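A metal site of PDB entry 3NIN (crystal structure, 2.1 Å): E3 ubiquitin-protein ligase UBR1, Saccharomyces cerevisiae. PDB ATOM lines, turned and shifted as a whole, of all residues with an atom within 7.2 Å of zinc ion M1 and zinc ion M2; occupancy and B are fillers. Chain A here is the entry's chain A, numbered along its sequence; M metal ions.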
ATOM      1  N   HIS A   4       6.585  16.432 -11.666  1.00  0.00           N
ATOM      2  CA  HIS A   4       6.455  16.560 -13.114  1.00  0.00           C
ATOM      3  C   HIS A   4       6.478  15.199 -13.824  1.00  0.00           C
ATOM      4  O   HIS A   4       6.469  15.118 -15.060  1.00  0.00           O
ATOM      5  CB  HIS A   4       7.548  17.479 -13.676  1.00  0.00           C
ATOM      6  CG  HIS A   4       7.636  18.809 -12.992  1.00  0.00           C
ATOM      7  ND1 HIS A   4       6.662  19.785 -13.131  1.00  0.00           N
ATOM      8  CD2 HIS A   4       8.581  19.342 -12.174  1.00  0.00           C
ATOM      9  CE1 HIS A   4       7.011  20.854 -12.422  1.00  0.00           C
ATOM     10  NE2 HIS A   4       8.168  20.609 -11.849  1.00  0.00           N
ATOM     11  N   LYS A   5       6.491  14.129 -13.033  1.00  0.00           N
ATOM     12  CA  LYS A   5       6.415  12.763 -13.543  1.00  0.00           C
ATOM     13  C   LYS A   5       5.084  12.514 -14.250  1.00  0.00           C
ATOM     14  O   LYS A   5       4.023  12.921 -13.775  1.00  0.00           O
ATOM     15  CB  LYS A   5       6.550  11.746 -12.415  1.00  0.00           C
ATOM     16  CG  LYS A   5       7.957  11.617 -11.843  1.00  0.00           C
ATOM     17  CD  LYS A   5       8.066  10.451 -10.857  1.00  0.00           C
ATOM     18  CE  LYS A   5       8.034   9.103 -11.558  1.00  0.00           C
ATOM     19  NZ  LYS A   5       8.162   7.968 -10.595  1.00  0.00           N
ATOM     20  N   HIS A   6       5.148  11.839 -15.404  1.00  0.00           N
ATOM     21  CA  HIS A   6       3.949  11.453 -16.139  1.00  0.00           C
ATOM     22  C   HIS A   6       4.076  10.024 -16.690  1.00  0.00           C
ATOM     23  O   HIS A   6       3.693   9.759 -17.831  1.00  0.00           O
ATOM     24  CB  HIS A   6       3.681  12.461 -17.262  1.00  0.00           C
ATOM     25  CG  HIS A   6       4.760  12.523 -18.290  1.00  0.00           C
ATOM     26  ND1 HIS A   6       4.835  11.618 -19.331  1.00  0.00           N
ATOM     27  CD2 HIS A   6       5.819  13.352 -18.431  1.00  0.00           C
ATOM     28  CE1 HIS A   6       5.897  11.896 -20.072  1.00  0.00           C
ATOM     29  NE2 HIS A   6       6.501  12.947 -19.552  1.00  0.00           N
ATOM     30  N   ARG A   9       2.181   7.821 -19.797  1.00  0.00           N
ATOM     31  CA  ARG A   9       1.443   8.695 -20.709  1.00  0.00           C
ATOM     32  C   ARG A   9       2.321   9.816 -21.242  1.00  0.00           C
ATOM     33  O   ARG A   9       3.498   9.891 -20.916  1.00  0.00           O
ATOM     34  CB  ARG A   9       0.170   9.259 -20.050  1.00  0.00           C
ATOM     35  CG  ARG A   9       0.393  10.022 -18.739  1.00  0.00           C
ATOM     36  CD  ARG A   9      -0.741  11.013 -18.454  1.00  0.00           C
ATOM     37  NE  ARG A   9      -0.455  12.331 -19.038  1.00  0.00           N
ATOM     38  CZ  ARG A   9      -1.139  13.448 -18.803  1.00  0.00           C
ATOM     39  NH1 ARG A   9      -2.190  13.440 -17.997  1.00  0.00           N
ATOM     40  NH2 ARG A   9      -0.768  14.585 -19.396  1.00  0.00           N
ATOM     41  N   ASN A  10       1.766  10.675 -22.081  1.00  0.00           N
ATOM     42  CA  ASN A  10       2.501  11.838 -22.561  1.00  0.00           C
ATOM     43  C   ASN A  10       2.558  12.918 -21.479  1.00  0.00           C
ATOM     44  O   ASN A  10       1.757  12.907 -20.538  1.00  0.00           O
ATOM     45  CB  ASN A  10       1.860  12.414 -23.827  1.00  0.00           C
ATOM     46  CG  ASN A  10       0.460  12.941 -23.582  1.00  0.00           C
ATOM     47  OD1 ASN A  10      -0.385  12.248 -23.020  1.00  0.00           O
ATOM     48  ND2 ASN A  10       0.213  14.178 -24.006  1.00  0.00           N
ATOM     49  N   CYS A  11       3.492  13.844 -21.624  1.00  0.00           N
ATOM     50  CA  CYS A  11       3.563  15.000 -20.747  1.00  0.00           C
ATOM     51  C   CYS A  11       2.424  15.980 -21.012  1.00  0.00           C
ATOM     52  O   CYS A  11       1.625  16.293 -20.116  1.00  0.00           O
ATOM     53  CB  CYS A  11       4.898  15.715 -20.878  1.00  0.00           C
ATOM     54  SG  CYS A  11       4.860  17.282 -20.052  1.00  0.00           S
ATOM     55  N   GLY A  12       2.354  16.488 -22.245  1.00  0.00           N
ATOM     56  CA  GLY A  12       1.260  17.350 -22.683  1.00  0.00           C
ATOM     57  C   GLY A  12       1.137  18.691 -21.980  1.00  0.00           C
ATOM     58  O   GLY A  12       0.090  19.338 -22.065  1.00  0.00           O
ATOM     59  N   ARG A  13       2.196  19.108 -21.287  1.00  0.00           N
ATOM     60  CA  ARG A  13       2.224  20.415 -20.630  1.00  0.00           C
ATOM     61  C   ARG A  13       2.088  21.505 -21.675  1.00  0.00           C
ATOM     62  O   ARG A  13       2.892  21.581 -22.605  1.00  0.00           O
ATOM     63  CB  ARG A  13       3.517  20.622 -19.827  1.00  0.00           C
ATOM     64  CG  ARG A  13       3.638  22.020 -19.222  1.00  0.00           C
ATOM     65  CD  ARG A  13       4.952  22.239 -18.478  1.00  0.00           C
ATOM     66  NE  ARG A  13       4.844  21.875 -17.060  1.00  0.00           N
ATOM     67  CZ  ARG A  13       4.485  22.714 -16.089  1.00  0.00           C
ATOM     68  NH1 ARG A  13       4.196  23.976 -16.369  1.00  0.00           N
ATOM     69  NH2 ARG A  13       4.420  22.277 -14.839  1.00  0.00           N
ATOM     70  N   PHE A  15       2.457  25.171 -22.921  1.00  0.00           N
ATOM     71  CA  PHE A  15       3.406  26.234 -22.630  1.00  0.00           C
ATOM     72  C   PHE A  15       2.697  27.536 -22.316  1.00  0.00           C
ATOM     73  O   PHE A  15       1.617  27.821 -22.848  1.00  0.00           O
ATOM     74  CB  PHE A  15       4.390  26.385 -23.782  1.00  0.00           C
ATOM     75  CG  PHE A  15       5.315  25.203 -23.934  1.00  0.00           C
ATOM     76  CD1 PHE A  15       6.414  25.060 -23.088  1.00  0.00           C
ATOM     77  CD2 PHE A  15       5.069  24.242 -24.902  1.00  0.00           C
ATOM     78  CE1 PHE A  15       7.256  23.954 -23.209  1.00  0.00           C
ATOM     79  CE2 PHE A  15       5.919  23.140 -25.038  1.00  0.00           C
ATOM     80  CZ  PHE A  15       7.018  22.997 -24.192  1.00  0.00           C
ATOM     81  N   VAL A  34       8.479  19.297 -29.648  1.00  0.00           N
ATOM     82  CA  VAL A  34       9.108  20.083 -28.568  1.00  0.00           C
ATOM     83  C   VAL A  34       9.060  19.388 -27.208  1.00  0.00           C
ATOM     84  O   VAL A  34       8.243  18.494 -26.985  1.00  0.00           O
ATOM     85  CB  VAL A  34       8.488  21.502 -28.433  1.00  0.00           C
ATOM     86  CG1 VAL A  34       8.831  22.363 -29.647  1.00  0.00           C
ATOM     87  CG2 VAL A  34       6.971  21.428 -28.214  1.00  0.00           C
ATOM     88  N   LEU A  35       9.938  19.834 -26.300  1.00  0.00           N
ATOM     89  CA  LEU A  35      10.040  19.313 -24.922  1.00  0.00           C
ATOM     90  C   LEU A  35      10.056  20.462 -23.916  1.00  0.00           C
ATOM     91  O   LEU A  35      10.751  21.453 -24.129  1.00  0.00           O
ATOM     92  CB  LEU A  35      11.343  18.510 -24.770  1.00  0.00           C
ATOM     93  CG  LEU A  35      11.481  17.177 -25.503  1.00  0.00           C
ATOM     94  CD1 LEU A  35      12.890  16.631 -25.393  1.00  0.00           C
ATOM     95  CD2 LEU A  35      10.474  16.167 -24.973  1.00  0.00           C
ATOM     96  N   CYS A  36       9.323  20.329 -22.813  1.00  0.00           N
ATOM     97  CA  CYS A  36       9.421  21.309 -21.722  1.00  0.00           C
ATOM     98  C   CYS A  36      10.748  21.150 -20.939  1.00  0.00           C
ATOM     99  O   CYS A  36      11.487  20.197 -21.186  1.00  0.00           O
ATOM    100  CB  CYS A  36       8.214  21.212 -20.784  1.00  0.00           C
ATOM    101  SG  CYS A  36       8.257  19.811 -19.638  1.00  0.00           S
ATOM    102  N   ILE A  37      11.038  22.053 -20.010  1.00  0.00           N
ATOM    103  CA  ILE A  37      12.277  21.986 -19.208  1.00  0.00           C
ATOM    104  C   ILE A  37      12.321  20.836 -18.204  1.00  0.00           C
ATOM    105  O   ILE A  37      13.396  20.347 -17.856  1.00  0.00           O
ATOM    106  CB  ILE A  37      12.621  23.300 -18.455  1.00  0.00           C
ATOM    107  CG1 ILE A  37      11.413  23.834 -17.685  1.00  0.00           C
ATOM    108  CG2 ILE A  37      13.221  24.325 -19.411  1.00  0.00           C
ATOM    109  CD1 ILE A  37      11.782  24.750 -16.523  1.00  0.00           C
ATOM    110  N   HIS A  38      11.150  20.421 -17.728  1.00  0.00           N
ATOM    111  CA  HIS A  38      11.080  19.371 -16.715  1.00  0.00           C
ATOM    112  C   HIS A  38      11.307  17.994 -17.349  1.00  0.00           C
ATOM    113  O   HIS A  38      11.632  17.033 -16.662  1.00  0.00           O
ATOM    114  CB  HIS A  38       9.743  19.444 -15.984  1.00  0.00           C
ATOM    115  CG  HIS A  38       9.436  20.801 -15.447  1.00  0.00           C
ATOM    116  ND1 HIS A  38       8.403  21.582 -15.927  1.00  0.00           N
ATOM    117  CD2 HIS A  38      10.035  21.530 -14.481  1.00  0.00           C
ATOM    118  CE1 HIS A  38       8.372  22.733 -15.278  1.00  0.00           C
ATOM    119  NE2 HIS A  38       9.359  22.732 -14.393  1.00  0.00           N
ATOM    120  N   CYS A  39      11.174  17.939 -18.672  1.00  0.00           N
ATOM    121  CA  CYS A  39      11.265  16.689 -19.415  1.00  0.00           C
ATOM    122  C   CYS A  39      12.572  16.524 -20.190  1.00  0.00           C
ATOM    123  O   CYS A  39      13.127  15.418 -20.254  1.00  0.00           O
ATOM    124  CB  CYS A  39      10.057  16.564 -20.340  1.00  0.00           C
ATOM    125  SG  CYS A  39       8.481  16.192 -19.479  1.00  0.00           S
ATOM    126  N   PHE A  40      13.077  17.596 -20.793  1.00  0.00           N
ATOM    127  CA  PHE A  40      14.308  17.531 -21.594  1.00  0.00           C
ATOM    128  C   PHE A  40      15.473  16.945 -20.778  1.00  0.00           C
ATOM    129  O   PHE A  40      15.869  17.506 -19.749  1.00  0.00           O
ATOM    130  CB  PHE A  40      14.685  18.897 -22.181  1.00  0.00           C
ATOM    131  CG  PHE A  40      16.008  18.909 -22.905  1.00  0.00           C
ATOM    132  CD1 PHE A  40      16.081  18.576 -24.261  1.00  0.00           C
ATOM    133  CD2 PHE A  40      17.187  19.260 -22.248  1.00  0.00           C
ATOM    134  CE1 PHE A  40      17.293  18.589 -24.948  1.00  0.00           C
ATOM    135  CE2 PHE A  40      18.424  19.265 -22.924  1.00  0.00           C
ATOM    136  CZ  PHE A  40      18.467  18.929 -24.269  1.00  0.00           C
ATOM    137  N   ILE A  62       2.114  22.170 -26.786  1.00  0.00           N
ATOM    138  CA  ILE A  62       2.375  21.256 -25.664  1.00  0.00           C
ATOM    139  C   ILE A  62       3.651  20.435 -25.838  1.00  0.00           C
ATOM    140  O   ILE A  62       4.055  20.150 -26.960  1.00  0.00           O
ATOM    141  CB  ILE A  62       1.186  20.269 -25.435  1.00  0.00           C
ATOM    142  CG1 ILE A  62       1.043  19.269 -26.592  1.00  0.00           C
ATOM    143  CG2 ILE A  62      -0.142  21.021 -25.171  1.00  0.00           C
ATOM    144  CD1 ILE A  62      -0.024  18.186 -26.373  1.00  0.00           C
ATOM    145  N   CYS A  63       4.257  20.062 -24.704  1.00  0.00           N
ATOM    146  CA  CYS A  63       5.399  19.163 -24.634  1.00  0.00           C
ATOM    147  C   CYS A  63       5.026  17.783 -25.194  1.00  0.00           C
ATOM    148  O   CYS A  63       3.979  17.236 -24.880  1.00  0.00           O
ATOM    149  CB  CYS A  63       5.902  19.059 -23.175  1.00  0.00           C
ATOM    150  SG  CYS A  63       7.201  17.833 -22.726  1.00  0.00           S
ATOM    151  N   ASP A  64       5.907  17.221 -26.032  1.00  0.00           N
ATOM    152  CA  ASP A  64       5.674  15.935 -26.679  1.00  0.00           C
ATOM    153  C   ASP A  64       6.371  14.748 -25.995  1.00  0.00           C
ATOM    154  O   ASP A  64       6.312  13.639 -26.506  1.00  0.00           O
ATOM    155  CB  ASP A  64       6.111  15.985 -28.151  1.00  0.00           C
ATOM    156  CG  ASP A  64       5.311  17.001 -28.965  1.00  0.00           C
ATOM    157  OD1 ASP A  64       4.107  16.793 -29.159  1.00  0.00           O
ATOM    158  OD2 ASP A  64       5.914  17.983 -29.430  1.00  0.00           O
ATOM    159  N   CYS A  65       7.052  14.997 -24.870  1.00  0.00           N
ATOM    160  CA  CYS A  65       7.678  13.918 -24.076  1.00  0.00           C
ATOM    161  C   CYS A  65       6.643  12.818 -23.813  1.00  0.00           C
ATOM    162  O   CYS A  65       5.574  13.075 -23.267  1.00  0.00           O
ATOM    163  CB  CYS A  65       8.243  14.460 -22.752  1.00  0.00           C
ATOM    164  SG  CYS A  65       8.981  13.254 -21.553  1.00  0.00           S
ATOM    165  N   GLY A  66       6.965  11.595 -24.251  1.00  0.00           N
ATOM    166  CA  GLY A  66       6.058  10.445 -24.088  1.00  0.00           C
ATOM    167  C   GLY A  66       5.115  10.178 -25.254  1.00  0.00           C
ATOM    168  O   GLY A  66       4.358   9.210 -25.224  1.00  0.00           O
ATOM    169  N   HIS A  76      14.231   9.456 -22.654  1.00  0.00           N
ATOM    170  CA  HIS A  76      14.293   9.084 -21.247  1.00  0.00           C
ATOM    171  C   HIS A  76      14.011  10.313 -20.406  1.00  0.00           C
ATOM    172  O   HIS A  76      14.881  11.147 -20.196  1.00  0.00           O
ATOM    173  CB  HIS A  76      15.641   8.447 -20.926  1.00  0.00           C
ATOM    174  CG  HIS A  76      15.978   7.291 -21.820  1.00  0.00           C
ATOM    175  ND1 HIS A  76      16.700   7.434 -22.985  1.00  0.00           N
ATOM    176  CD2 HIS A  76      15.660   5.971 -21.733  1.00  0.00           C
ATOM    177  CE1 HIS A  76      16.819   6.265 -23.569  1.00  0.00           C
ATOM    178  NE2 HIS A  76      16.206   5.362 -22.832  1.00  0.00           N
ATOM    179  N   CYS A  77      12.768  10.410 -19.945  1.00  0.00           N
ATOM    180  CA  CYS A  77      12.249  11.607 -19.300  1.00  0.00           C
ATOM    181  C   CYS A  77      13.050  11.995 -18.055  1.00  0.00           C
ATOM    182  O   CYS A  77      13.298  11.156 -17.191  1.00  0.00           O
ATOM    183  CB  CYS A  77      10.770  11.427 -18.950  1.00  0.00           C
ATOM    184  SG  CYS A  77      10.050  12.830 -18.084  1.00  0.00           S
ATOM    185  N   LYS A  78      13.447  13.263 -17.985  1.00  0.00           N
ATOM    186  CA  LYS A  78      14.234  13.780 -16.874  1.00  0.00           C
ATOM    187  C   LYS A  78      13.502  13.674 -15.534  1.00  0.00           C
ATOM    188  O   LYS A  78      14.113  13.374 -14.511  1.00  0.00           O
ATOM    189  CB  LYS A  78      14.661  15.229 -17.119  1.00  0.00           C
ATOM    190  CG  LYS A  78      15.555  15.808 -16.019  1.00  0.00           C
ATOM    191  CD  LYS A  78      16.383  16.969 -16.514  1.00  0.00           C
ATOM    192  CE  LYS A  78      16.698  17.948 -15.383  1.00  0.00           C
ATOM    193  NZ  LYS A  78      15.507  18.792 -15.062  1.00  0.00           N
ATOM    194  N   ALA A  79      12.192  13.923 -15.569  1.00  0.00           N
ATOM    195  CA  ALA A  79      11.350  13.838 -14.376  1.00  0.00           C
ATOM    196  C   ALA A  79      11.337  12.438 -13.744  1.00  0.00           C
ATOM    197  O   ALA A  79      11.039  12.295 -12.556  1.00  0.00           O
ATOM    198  CB  ALA A  79       9.929  14.305 -14.682  1.00  0.00           C
ATOM    199  N   GLU A  80      11.645  11.419 -14.547  1.00  0.00           N
ATOM    200  CA  GLU A  80      11.713  10.035 -14.062  1.00  0.00           C
ATOM    201  C   GLU A  80      12.931   9.803 -13.153  1.00  0.00           C
ATOM    202  O   GLU A  80      12.867   8.972 -12.243  1.00  0.00           O
ATOM    203  CB  GLU A  80      11.736   9.040 -15.230  1.00  0.00           C
ATOM    204  CG  GLU A  80      10.448   8.978 -16.061  1.00  0.00           C
ATOM    205  CD  GLU A  80       9.289   8.311 -15.337  1.00  0.00           C
ATOM    206  OE1 GLU A  80       9.517   7.599 -14.333  1.00  0.00           O
ATOM    207  OE2 GLU A  80       8.137   8.486 -15.786  1.00  0.00           O
HETATM  208 ZN    ZN M   1       8.567  13.918 -19.625  1.00  0.00          ZN
HETATM  209 ZN    ZN M   2       7.125  17.975 -20.537  1.00  0.00          ZN
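Four residues have an atom within 4 Å of zinc ion M2: Cys 11, Cys 36, Cys 39 and Cys 63.
The backbone carbonyl oxygen (O) of Cys 65 is in hydrogen-bond range of the backbone NH (N) of Cys 11 (2.8 Å). The backbone carbonyl oxygen (O) of Arg 13 sits at hydrogen-bond distance from the backbone NH (N) of Cys 63 (2.9 Å). The backbone carbonyl oxygen (O) of Cys 63 sits at hydrogen-bond distance from the backbone NH (N) of Gly 12, 3.2 Å away. The backbone NH (N) of Cys 11 lies close to a ring nitrogen (ND1) of His 6. ND1 of His 6 is in hydrogen-bond range of O of Arg 9 (2.7 Å). SG of Cys 77 lies close to N of Ala 79 (3.5 Å). The side-chain sulfur of Cys 11 lies close to the backbone NH of Arg 13. NH2 of Arg 9 is in hydrogen-bond range of O of Cys 11 (3.0 Å).
Of the 26 residues printed, 4 come within 4 Å of zinc ion M1. The nearest printed residue that does not touch zinc ion M1 is Cys 11 (4.3 Å).
Zinc ion M2 is bound by the side-chain sulfur of Cys 63, the side-chain sulfur of Cys 36, the side-chain sulfur of Cys 11 and the side-chain sulfur of Cys 39.
Zinc ion M1 is bound by the side-chain sulfur of Cys 65, the side-chain sulfur of Cys 39, a ring nitrogen (NE2) of His 6 and the side-chain sulfur of Cys 77. Zinc ion M1 has four donor atoms within binding distance.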
